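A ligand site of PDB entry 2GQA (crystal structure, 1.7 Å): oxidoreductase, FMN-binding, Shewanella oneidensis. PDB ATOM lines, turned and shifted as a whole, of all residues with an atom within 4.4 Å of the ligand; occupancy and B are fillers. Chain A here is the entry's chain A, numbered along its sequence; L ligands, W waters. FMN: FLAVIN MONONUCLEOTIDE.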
ATOM      1  N   PRO A  23     -21.468  -6.738  32.213  1.00  0.00           N
ATOM      2  CA  PRO A  23     -21.231  -6.495  30.794  1.00  0.00           C
ATOM      3  C   PRO A  23     -21.522  -7.721  29.944  1.00  0.00           C
ATOM      4  O   PRO A  23     -21.579  -8.832  30.462  1.00  0.00           O
ATOM      5  CB  PRO A  23     -19.753  -6.097  30.756  1.00  0.00           C
ATOM      6  CG  PRO A  23     -19.178  -6.991  31.804  1.00  0.00           C
ATOM      7  CD  PRO A  23     -20.195  -6.942  32.927  1.00  0.00           C
ATOM      8  N   PRO A  24     -21.703  -7.514  28.633  1.00  0.00           N
ATOM      9  CA  PRO A  24     -21.997  -8.615  27.708  1.00  0.00           C
ATOM     10  C   PRO A  24     -20.835  -9.597  27.673  1.00  0.00           C
ATOM     11  O   PRO A  24     -19.682  -9.200  27.458  1.00  0.00           O
ATOM     12  CB  PRO A  24     -22.203  -7.890  26.375  1.00  0.00           C
ATOM     13  CG  PRO A  24     -21.341  -6.673  26.495  1.00  0.00           C
ATOM     14  CD  PRO A  24     -21.580  -6.230  27.918  1.00  0.00           C
ATOM     15  N   MET A  25     -21.141 -10.871  27.898  1.00  0.00           N
ATOM     16  CA  MET A  25     -20.115 -11.902  27.899  1.00  0.00           C
ATOM     17  C   MET A  25     -20.557 -13.208  27.255  1.00  0.00           C
ATOM     18  O   MET A  25     -21.392 -13.940  27.794  1.00  0.00           O
ATOM     19  CB  MET A  25     -19.620 -12.168  29.325  1.00  0.00           C
ATOM     20  CG  MET A  25     -18.849 -11.000  29.917  1.00  0.00           C
ATOM     21  SD  MET A  25     -18.211 -11.331  31.567  1.00  0.00           S
ATOM     22  CE  MET A  25     -19.772 -11.390  32.538  1.00  0.00           C
ATOM     23  N   THR A  26     -19.982 -13.490  26.089  1.00  0.00           N
ATOM     24  CA  THR A  26     -20.245 -14.699  25.326  1.00  0.00           C
ATOM     25  C   THR A  26     -19.873 -15.921  26.151  1.00  0.00           C
ATOM     26  O   THR A  26     -18.754 -16.017  26.634  1.00  0.00           O
ATOM     27  CB  THR A  26     -19.397 -14.695  24.037  1.00  0.00           C
ATOM     28  OG1 THR A  26     -19.864 -13.657  23.165  1.00  0.00           O
ATOM     29  CG2 THR A  26     -19.489 -16.036  23.310  1.00  0.00           C
ATOM     30  N   ARG A  27     -20.811 -16.860  26.321  1.00  0.00           N
ATOM     31  CA  ARG A  27     -20.554 -18.088  27.075  1.00  0.00           C
ATOM     32  C   ARG A  27     -20.742 -19.326  26.184  1.00  0.00           C
ATOM     33  O   ARG A  27     -20.416 -20.450  26.590  1.00  0.00           O
ATOM     34  CB  ARG A  27     -21.476 -18.184  28.296  1.00  0.00           C
ATOM     35  CG  ARG A  27     -21.379 -17.008  29.272  1.00  0.00           C
ATOM     36  CD  ARG A  27     -19.937 -16.698  29.687  1.00  0.00           C
ATOM     37  NE  ARG A  27     -19.270 -17.855  30.275  1.00  0.00           N
ATOM     38  CZ  ARG A  27     -19.412 -18.251  31.542  1.00  0.00           C
ATOM     39  NH1 ARG A  27     -20.198 -17.585  32.376  1.00  0.00           N
ATOM     40  NH2 ARG A  27     -18.794 -19.348  31.970  1.00  0.00           N
ATOM     41  N   GLU A  57     -24.984 -11.472  26.616  1.00  0.00           N
ATOM     42  CA  GLU A  57     -23.855 -11.823  25.776  1.00  0.00           C
ATOM     43  C   GLU A  57     -24.300 -11.457  24.364  1.00  0.00           C
ATOM     44  O   GLU A  57     -25.500 -11.392  24.080  1.00  0.00           O
ATOM     45  CB  GLU A  57     -23.650 -13.329  25.859  1.00  0.00           C
ATOM     46  CG  GLU A  57     -24.919 -14.097  25.479  1.00  0.00           C
ATOM     47  CD  GLU A  57     -24.999 -15.452  26.134  1.00  0.00           C
ATOM     48  OE1 GLU A  57     -24.417 -16.406  25.591  1.00  0.00           O
ATOM     49  OE2 GLU A  57     -25.634 -15.552  27.199  1.00  0.00           O
ATOM     50  N   GLY A  58     -23.340 -11.247  23.473  1.00  0.00           N
ATOM     51  CA  GLY A  58     -23.697 -10.921  22.106  1.00  0.00           C
ATOM     52  C   GLY A  58     -24.640 -11.952  21.510  1.00  0.00           C
ATOM     53  O   GLY A  58     -24.451 -13.160  21.679  1.00  0.00           O
ATOM     54  N   GLN A 100     -27.556  -7.571  23.691  1.00  0.00           N
ATOM     55  CA  GLN A 100     -26.500  -6.996  22.859  1.00  0.00           C
ATOM     56  C   GLN A 100     -26.623  -7.562  21.439  1.00  0.00           C
ATOM     57  O   GLN A 100     -26.294  -8.720  21.207  1.00  0.00           O
ATOM     58  CB  GLN A 100     -25.107  -7.311  23.405  1.00  0.00           C
ATOM     59  CG  GLN A 100     -24.030  -6.595  22.565  1.00  0.00           C
ATOM     60  CD  GLN A 100     -22.607  -6.980  22.899  1.00  0.00           C
ATOM     61  OE1 GLN A 100     -22.220  -8.135  22.796  1.00  0.00           O
ATOM     62  NE2 GLN A 100     -21.800  -5.993  23.293  1.00  0.00           N
ATOM     63  N   TRP A 102     -25.607  -8.371  17.890  1.00  0.00           N
ATOM     64  CA  TRP A 102     -24.303  -8.659  17.326  1.00  0.00           C
ATOM     65  C   TRP A 102     -24.192  -9.024  15.852  1.00  0.00           C
ATOM     66  O   TRP A 102     -25.021  -9.752  15.305  1.00  0.00           O
ATOM     67  CB  TRP A 102     -23.753  -9.828  18.156  1.00  0.00           C
ATOM     68  CG  TRP A 102     -22.271  -9.994  18.247  1.00  0.00           C
ATOM     69  CD1 TRP A 102     -21.303  -9.086  17.889  1.00  0.00           C
ATOM     70  CD2 TRP A 102     -21.589 -11.099  18.844  1.00  0.00           C
ATOM     71  NE1 TRP A 102     -20.062  -9.565  18.250  1.00  0.00           N
ATOM     72  CE2 TRP A 102     -20.216 -10.796  18.841  1.00  0.00           C
ATOM     73  CE3 TRP A 102     -22.021 -12.309  19.392  1.00  0.00           C
ATOM     74  CZ2 TRP A 102     -19.249 -11.675  19.370  1.00  0.00           C
ATOM     75  CZ3 TRP A 102     -21.070 -13.178  19.926  1.00  0.00           C
ATOM     76  CH2 TRP A 102     -19.700 -12.852  19.904  1.00  0.00           C
ATOM     77  N   HIS A 181     -23.572  -3.681  19.532  1.00  0.00           N
ATOM     78  CA  HIS A 181     -22.156  -4.015  19.664  1.00  0.00           C
ATOM     79  C   HIS A 181     -21.418  -3.394  18.499  1.00  0.00           C
ATOM     80  O   HIS A 181     -21.370  -3.959  17.405  1.00  0.00           O
ATOM     81  CB  HIS A 181     -21.928  -5.535  19.656  1.00  0.00           C
ATOM     82  CG  HIS A 181     -20.580  -5.933  20.168  1.00  0.00           C
ATOM     83  ND1 HIS A 181     -19.540  -5.047  20.299  1.00  0.00           N
ATOM     84  CD2 HIS A 181     -20.116  -7.131  20.613  1.00  0.00           C
ATOM     85  CE1 HIS A 181     -18.489  -5.671  20.810  1.00  0.00           C
ATOM     86  NE2 HIS A 181     -18.814  -6.923  21.011  1.00  0.00           N
ATOM     87  N   ASN A 184     -15.111  -3.919  19.932  1.00  0.00           N
ATOM     88  CA  ASN A 184     -14.232  -5.078  19.874  1.00  0.00           C
ATOM     89  C   ASN A 184     -13.954  -5.695  18.513  1.00  0.00           C
ATOM     90  O   ASN A 184     -13.925  -6.923  18.362  1.00  0.00           O
ATOM     91  CB  ASN A 184     -14.707  -6.119  20.884  1.00  0.00           C
ATOM     92  CG  ASN A 184     -14.723  -5.570  22.301  1.00  0.00           C
ATOM     93  OD1 ASN A 184     -14.104  -4.536  22.563  1.00  0.00           O
ATOM     94  ND2 ASN A 184     -15.427  -6.234  23.202  1.00  0.00           N
ATOM     95  N   ARG A 233     -22.172   0.181  22.286  1.00  0.00           N
ATOM     96  CA  ARG A 233     -20.853  -0.105  22.855  1.00  0.00           C
ATOM     97  C   ARG A 233     -19.744   0.195  21.844  1.00  0.00           C
ATOM     98  O   ARG A 233     -19.830  -0.206  20.685  1.00  0.00           O
ATOM     99  CB  ARG A 233     -20.751  -1.571  23.305  1.00  0.00           C
ATOM    100  CG  ARG A 233     -19.576  -1.785  24.275  1.00  0.00           C
ATOM    101  CD  ARG A 233     -19.466  -3.208  24.809  1.00  0.00           C
ATOM    102  NE  ARG A 233     -18.910  -3.187  26.162  1.00  0.00           N
ATOM    103  CZ  ARG A 233     -18.232  -4.182  26.746  1.00  0.00           C
ATOM    104  NH1 ARG A 233     -17.999  -5.317  26.104  1.00  0.00           N
ATOM    105  NH2 ARG A 233     -17.793  -4.038  27.984  1.00  0.00           N
ATOM    106  N   VAL A 272     -11.072  -2.402  28.196  1.00  0.00           N
ATOM    107  CA  VAL A 272     -10.099  -3.489  28.156  1.00  0.00           C
ATOM    108  C   VAL A 272     -10.767  -4.654  27.451  1.00  0.00           C
ATOM    109  O   VAL A 272     -11.971  -4.870  27.588  1.00  0.00           O
ATOM    110  CB  VAL A 272      -9.716  -3.957  29.591  1.00  0.00           C
ATOM    111  CG1 VAL A 272      -8.809  -5.210  29.508  1.00  0.00           C
ATOM    112  CG2 VAL A 272      -9.026  -2.836  30.339  1.00  0.00           C
ATOM    113  N   ASP A 273      -9.990  -5.384  26.647  1.00  0.00           N
ATOM    114  CA  ASP A 273     -10.517  -6.574  26.003  1.00  0.00           C
ATOM    115  C   ASP A 273      -9.456  -7.627  26.305  1.00  0.00           C
ATOM    116  O   ASP A 273      -8.349  -7.564  25.780  1.00  0.00           O
ATOM    117  CB  ASP A 273     -10.682  -6.378  24.498  1.00  0.00           C
ATOM    118  CG  ASP A 273     -11.678  -7.375  23.899  1.00  0.00           C
ATOM    119  OD1 ASP A 273     -11.558  -7.700  22.706  1.00  0.00           O
ATOM    120  OD2 ASP A 273     -12.600  -7.821  24.638  1.00  0.00           O
ATOM    121  N   TRP A 274      -9.827  -8.574  27.165  1.00  0.00           N
ATOM    122  CA  TRP A 274      -8.941  -9.639  27.612  1.00  0.00           C
ATOM    123  C   TRP A 274      -7.677  -9.035  28.202  1.00  0.00           C
ATOM    124  O   TRP A 274      -7.758  -8.428  29.266  1.00  0.00           O
ATOM    125  CB  TRP A 274      -8.644 -10.602  26.462  1.00  0.00           C
ATOM    126  CG  TRP A 274      -9.910 -11.260  26.015  1.00  0.00           C
ATOM    127  CD1 TRP A 274     -10.659 -10.955  24.916  1.00  0.00           C
ATOM    128  CD2 TRP A 274     -10.668 -12.247  26.745  1.00  0.00           C
ATOM    129  NE1 TRP A 274     -11.832 -11.678  24.918  1.00  0.00           N
ATOM    130  CE2 TRP A 274     -11.864 -12.478  26.033  1.00  0.00           C
ATOM    131  CE3 TRP A 274     -10.444 -12.953  27.938  1.00  0.00           C
ATOM    132  CZ2 TRP A 274     -12.834 -13.388  26.464  1.00  0.00           C
ATOM    133  CZ3 TRP A 274     -11.422 -13.857  28.372  1.00  0.00           C
ATOM    134  CH2 TRP A 274     -12.599 -14.068  27.636  1.00  0.00           C
ATOM    135  N   ALA A 299     -16.175  -0.501  31.196  1.00  0.00           N
ATOM    136  CA  ALA A 299     -15.875  -1.849  31.689  1.00  0.00           C
ATOM    137  C   ALA A 299     -14.441  -2.180  31.263  1.00  0.00           C
ATOM    138  O   ALA A 299     -14.019  -1.826  30.162  1.00  0.00           O
ATOM    139  CB  ALA A 299     -16.850  -2.881  31.113  1.00  0.00           C
ATOM    140  N   GLY A 300     -13.704  -2.853  32.143  1.00  0.00           N
ATOM    141  CA  GLY A 300     -12.342  -3.231  31.828  1.00  0.00           C
ATOM    142  C   GLY A 300     -11.409  -3.116  33.015  1.00  0.00           C
ATOM    143  O   GLY A 300     -10.936  -2.038  33.354  1.00  0.00           O
ATOM    144  N   ARG A 301     -11.163  -4.254  33.663  1.00  0.00           N
ATOM    145  CA  ARG A 301     -10.274  -4.344  34.808  1.00  0.00           C
ATOM    146  C   ARG A 301     -10.616  -3.443  35.987  1.00  0.00           C
ATOM    147  O   ARG A 301      -9.725  -2.976  36.698  1.00  0.00           O
ATOM    148  CB  ARG A 301      -8.829  -4.081  34.385  1.00  0.00           C
ATOM    149  CG  ARG A 301      -8.251  -5.141  33.450  1.00  0.00           C
ATOM    150  CD  ARG A 301      -8.292  -6.528  34.061  1.00  0.00           C
ATOM    151  NE  ARG A 301      -7.488  -7.497  33.306  1.00  0.00           N
ATOM    152  CZ  ARG A 301      -7.558  -8.815  33.460  1.00  0.00           C
ATOM    153  NH1 ARG A 301      -8.394  -9.347  34.336  1.00  0.00           N
ATOM    154  NH2 ARG A 301      -6.767  -9.602  32.742  1.00  0.00           N
ATOM    155  N   GLY A 320     -19.005  -1.631  34.531  1.00  0.00           N
ATOM    156  CA  GLY A 320     -19.233  -3.048  34.307  1.00  0.00           C
ATOM    157  C   GLY A 320     -18.062  -3.869  34.833  1.00  0.00           C
ATOM    158  O   GLY A 320     -16.910  -3.428  34.788  1.00  0.00           O
ATOM    159  N   PHE A 321     -18.368  -5.043  35.378  1.00  0.00           N
ATOM    160  CA  PHE A 321     -17.361  -5.959  35.913  1.00  0.00           C
ATOM    161  C   PHE A 321     -17.636  -7.266  35.168  1.00  0.00           C
ATOM    162  O   PHE A 321     -18.661  -7.892  35.373  1.00  0.00           O
ATOM    163  CB  PHE A 321     -17.557  -6.170  37.427  1.00  0.00           C
ATOM    164  CG  PHE A 321     -17.407  -4.906  38.227  1.00  0.00           C
ATOM    165  CD1 PHE A 321     -16.190  -4.593  38.833  1.00  0.00           C
ATOM    166  CD2 PHE A 321     -18.476  -4.031  38.385  1.00  0.00           C
ATOM    167  CE1 PHE A 321     -16.032  -3.438  39.582  1.00  0.00           C
ATOM    168  CE2 PHE A 321     -18.323  -2.860  39.125  1.00  0.00           C
ATOM    169  CZ  PHE A 321     -17.103  -2.561  39.730  1.00  0.00           C
ATOM    170  N   GLY A 322     -16.716  -7.653  34.303  1.00  0.00           N
ATOM    171  CA  GLY A 322     -16.921  -8.855  33.513  1.00  0.00           C
ATOM    172  C   GLY A 322     -16.474 -10.150  34.144  1.00  0.00           C
ATOM    173  O   GLY A 322     -17.278 -10.904  34.673  1.00  0.00           O
ATOM    174  N   ARG A 323     -15.177 -10.409  34.065  1.00  0.00           N
ATOM    175  CA  ARG A 323     -14.631 -11.621  34.631  1.00  0.00           C
ATOM    176  C   ARG A 323     -15.044 -11.841  36.083  1.00  0.00           C
ATOM    177  O   ARG A 323     -15.378 -12.957  36.462  1.00  0.00           O
ATOM    178  CB  ARG A 323     -13.124 -11.637  34.412  1.00  0.00           C
ATOM    179  CG  ARG A 323     -12.849 -11.989  32.943  1.00  0.00           C
ATOM    180  CD  ARG A 323     -11.447 -11.646  32.455  1.00  0.00           C
ATOM    181  NE  ARG A 323     -11.303 -10.231  32.129  1.00  0.00           N
ATOM    182  CZ  ARG A 323     -10.253  -9.724  31.492  1.00  0.00           C
ATOM    183  NH1 ARG A 323     -10.199  -8.424  31.216  1.00  0.00           N
ATOM    184  NH2 ARG A 323      -9.256 -10.521  31.110  1.00  0.00           N
ATOM    185  N   PRO A 324     -15.063 -10.776  36.908  1.00  0.00           N
ATOM    186  CA  PRO A 324     -15.485 -11.012  38.288  1.00  0.00           C
ATOM    187  C   PRO A 324     -16.937 -11.492  38.385  1.00  0.00           C
ATOM    188  O   PRO A 324     -17.273 -12.277  39.277  1.00  0.00           O
ATOM    189  CB  PRO A 324     -15.298  -9.646  38.947  1.00  0.00           C
ATOM    190  CG  PRO A 324     -14.099  -9.093  38.208  1.00  0.00           C
ATOM    191  CD  PRO A 324     -14.437  -9.449  36.770  1.00  0.00           C
ATOM    192  N   ILE A 326     -18.413 -13.433  36.279  1.00  0.00           N
ATOM    193  CA  ILE A 326     -18.477 -14.826  35.853  1.00  0.00           C
ATOM    194  C   ILE A 326     -18.394 -15.722  37.096  1.00  0.00           C
ATOM    195  O   ILE A 326     -19.196 -16.639  37.290  1.00  0.00           O
ATOM    196  CB  ILE A 326     -17.269 -15.191  34.936  1.00  0.00           C
ATOM    197  CG1 ILE A 326     -17.283 -14.344  33.660  1.00  0.00           C
ATOM    198  CG2 ILE A 326     -17.272 -16.705  34.641  1.00  0.00           C
ATOM    199  CD1 ILE A 326     -18.201 -14.829  32.570  1.00  0.00           C
ATOM    200  N   LEU A 349     -15.178 -21.009  30.220  1.00  0.00           N
ATOM    201  CA  LEU A 349     -15.814 -19.783  29.774  1.00  0.00           C
ATOM    202  C   LEU A 349     -16.719 -20.050  28.569  1.00  0.00           C
ATOM    203  O   LEU A 349     -17.825 -19.516  28.497  1.00  0.00           O
ATOM    204  CB  LEU A 349     -14.778 -18.744  29.384  1.00  0.00           C
ATOM    205  CG  LEU A 349     -14.001 -18.110  30.535  1.00  0.00           C
ATOM    206  CD1 LEU A 349     -12.894 -17.207  30.001  1.00  0.00           C
ATOM    207  CD2 LEU A 349     -14.974 -17.325  31.432  1.00  0.00           C
ATOM    208  N   PHE A 350     -16.247 -20.862  27.629  1.00  0.00           N
ATOM    209  CA  PHE A 350     -17.017 -21.147  26.415  1.00  0.00           C
ATOM    210  C   PHE A 350     -17.378 -22.606  26.217  1.00  0.00           C
ATOM    211  O   PHE A 350     -16.554 -23.503  26.432  1.00  0.00           O
ATOM    212  CB  PHE A 350     -16.226 -20.690  25.183  1.00  0.00           C
ATOM    213  CG  PHE A 350     -15.652 -19.317  25.324  1.00  0.00           C
ATOM    214  CD1 PHE A 350     -14.300 -19.130  25.538  1.00  0.00           C
ATOM    215  CD2 PHE A 350     -16.479 -18.203  25.291  1.00  0.00           C
ATOM    216  CE1 PHE A 350     -13.770 -17.856  25.717  1.00  0.00           C
ATOM    217  CE2 PHE A 350     -15.960 -16.923  25.463  1.00  0.00           C
ATOM    218  CZ  PHE A 350     -14.602 -16.750  25.686  1.00  0.00           C
HETATM  219  N1  FMN L   1     -17.823  -8.057  25.198  1.00  0.00           N
HETATM  220  C2  FMN L   1     -18.904  -7.795  24.329  1.00  0.00           C
HETATM  221  O2  FMN L   1     -19.184  -6.682  23.971  1.00  0.00           O
HETATM  222  N3  FMN L   1     -19.721  -8.920  23.930  1.00  0.00           N
HETATM  223  C4  FMN L   1     -19.444 -10.237  24.172  1.00  0.00           C
HETATM  224  O4  FMN L   1     -20.233 -11.106  23.854  1.00  0.00           O
HETATM  225  C4A FMN L   1     -18.194 -10.519  24.907  1.00  0.00           C
HETATM  226  N5  FMN L   1     -17.791 -11.817  25.187  1.00  0.00           N
HETATM  227  C5A FMN L   1     -16.965 -11.992  26.281  1.00  0.00           C
HETATM  228  C6  FMN L   1     -16.937 -13.369  26.852  1.00  0.00           C
HETATM  229  C7  FMN L   1     -16.220 -13.623  28.088  1.00  0.00           C
HETATM  230  C7M FMN L   1     -16.187 -15.024  28.687  1.00  0.00           C
HETATM  231  C8  FMN L   1     -15.582 -12.535  28.787  1.00  0.00           C
HETATM  232  C8M FMN L   1     -14.728 -12.584  30.080  1.00  0.00           C
HETATM  233  C9  FMN L   1     -15.501 -11.266  28.126  1.00  0.00           C
HETATM  234  C9A FMN L   1     -16.263 -10.886  26.984  1.00  0.00           C
HETATM  235  N10 FMN L   1     -16.561  -9.568  26.446  1.00  0.00           N
HETATM  236  C10 FMN L   1     -17.473  -9.311  25.454  1.00  0.00           C
HETATM  237  C1' FMN L   1     -15.798  -8.395  27.041  1.00  0.00           C
HETATM  238  C2' FMN L   1     -16.447  -7.962  28.352  1.00  0.00           C
HETATM  239  O2' FMN L   1     -17.770  -7.441  28.186  1.00  0.00           O
HETATM  240  C3' FMN L   1     -15.646  -6.902  29.106  1.00  0.00           C
HETATM  241  O3' FMN L   1     -15.638  -5.665  28.370  1.00  0.00           O
HETATM  242  C4' FMN L   1     -14.221  -7.334  29.354  1.00  0.00           C
HETATM  243  O4' FMN L   1     -14.142  -8.686  29.912  1.00  0.00           O
HETATM  244  C5' FMN L   1     -13.460  -6.353  30.229  1.00  0.00           C
HETATM  245  O5' FMN L   1     -13.991  -6.303  31.597  1.00  0.00           O
HETATM  246  P   FMN L   1     -13.370  -7.148  32.791  1.00  0.00           P
HETATM  247  O1P FMN L   1     -13.636  -8.588  32.577  1.00  0.00           O
HETATM  248  O2P FMN L   1     -11.897  -6.784  32.847  1.00  0.00           O
HETATM  249  O3P FMN L   1     -14.129  -6.627  34.046  1.00  0.00           O
HETATM  250  O   HOH W   1     -14.275  -4.010  34.696  1.00  0.00           O
HETATM  251  O   HOH W   2     -12.854  -6.465  36.535  1.00  0.00           O
HETATM  252  O   HOH W   3     -14.088  -5.851  26.062  1.00  0.00           O
HETATM  253  O   HOH W   4     -12.218  -9.760  28.231  1.00  0.00           O
HETATM  254  O   HOH W   5     -14.576  -9.627  23.780  1.00  0.00           O
HETATM  255  O   HOH W   6     -10.799  -8.295  34.966  1.00  0.00           O
HETATM  256  O   HOH W   7     -16.856  -8.843  22.249  1.00  0.00           O
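The backbone carbonyl oxygen of Trp 274 sits at hydrogen-bond distance from the guanidinium group of Arg 323 (3.1 Å). The backbone carbonyl oxygen of Leu 349 lies within hydrogen-bond range of the guanidinium group of Arg 27, 2.8 Å away. N of Gly 58 lies close to OE1 of Gln 100.
Water W1 lies within hydrogen-bond range of the backbone carbonyl oxygen of Gly 320 (2.7 Å), an oxygen (O3P) of the ligand (2.7 Å), the backbone NH of Gly 300 (2.9 Å) and the backbone NH of Arg 301 (3.3 Å). Water W4 lies within hydrogen-bond range of O4' of the ligand (2.8 Å) and N of Trp 274 (2.9 Å). Water W3 lies within hydrogen-bond range of O3' of the ligand, O of Val 272, OD2 of Asp 273 and ND2 of Asn 184. Water W6 lies within hydrogen-bond range of NH1 of Arg 301, O2P of the ligand and NE of Arg 323. Water W7 lies within hydrogen-bond range of a ring nitrogen (NE2) of His 181, the side-chain amide nitrogen of Asn 184 and a nitrogen (N1) of the ligand.
Pro 23 touches the ligand (CB to O2', 3.5 Å). Met 25 touches the ligand. Asn 184 touches the ligand. O of Val 272 touches C5' of the ligand, at 3.4 Å. Trp 274 touches the ligand (CH2 to C8, 3.5 Å). Gly 300 touches the ligand (CA to O5', 3.5 Å). C of Phe 321 touches O3P of the ligand, 3.7 Å away. Pro 324 touches the ligand. CD2 of Leu 349 touches C7M of the ligand, at 3.8 Å. Phe 350 touches the ligand (CE2 to C7M, 3.7 Å). Hydrophobic or aromatic side chains that line the ligand: Pro 23, Pro 24, Met 25, His 181, Trp 274, Pro 324, Leu 349 and Phe 350. The nearest printed residue that does not touch the ligand is Asp 273 (4.04 Å).
NH1 of Arg 323 is in salt-bridge range of O2P of the ligand, at 2.9 Å. An oxygen (O2') of the ligand lies within hydrogen-bond range of the backbone carbonyl oxygen (O) of Pro 24 (2.7 Å). A ring nitrogen (NE2) of His 181 is in hydrogen-bond range of an oxygen (O2) of the ligand (3.0 Å). The backbone NH (N) of Arg 301 is in hydrogen-bond range of an oxygen (O2P) of the ligand, 2.8 Å away. The backbone NH of Arg 323 lies within hydrogen-bond range of an oxygen (O1P) of the ligand (2.8 Å). N of Gly 322 sits at hydrogen-bond distance from O3P of the ligand, at 2.8 Å. The backbone NH of Gly 58 sits at hydrogen-bond distance from an oxygen (O4) of the ligand (3.1 Å). O2 of the ligand sits at hydrogen-bond distance from NE2 of Gln 100. A nitrogen (N5) of the ligand sits at hydrogen-bond distance from the backbone NH (N) of Thr 26, at 2.9 Å. An oxygen (O4) of the ligand is in hydrogen-bond range of the side-chain hydroxyl (OG1) of Thr 26 (2.7 Å). NH2 of Arg 233 is in hydrogen-bond range of O3' of the ligand, at 2.7 Å.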
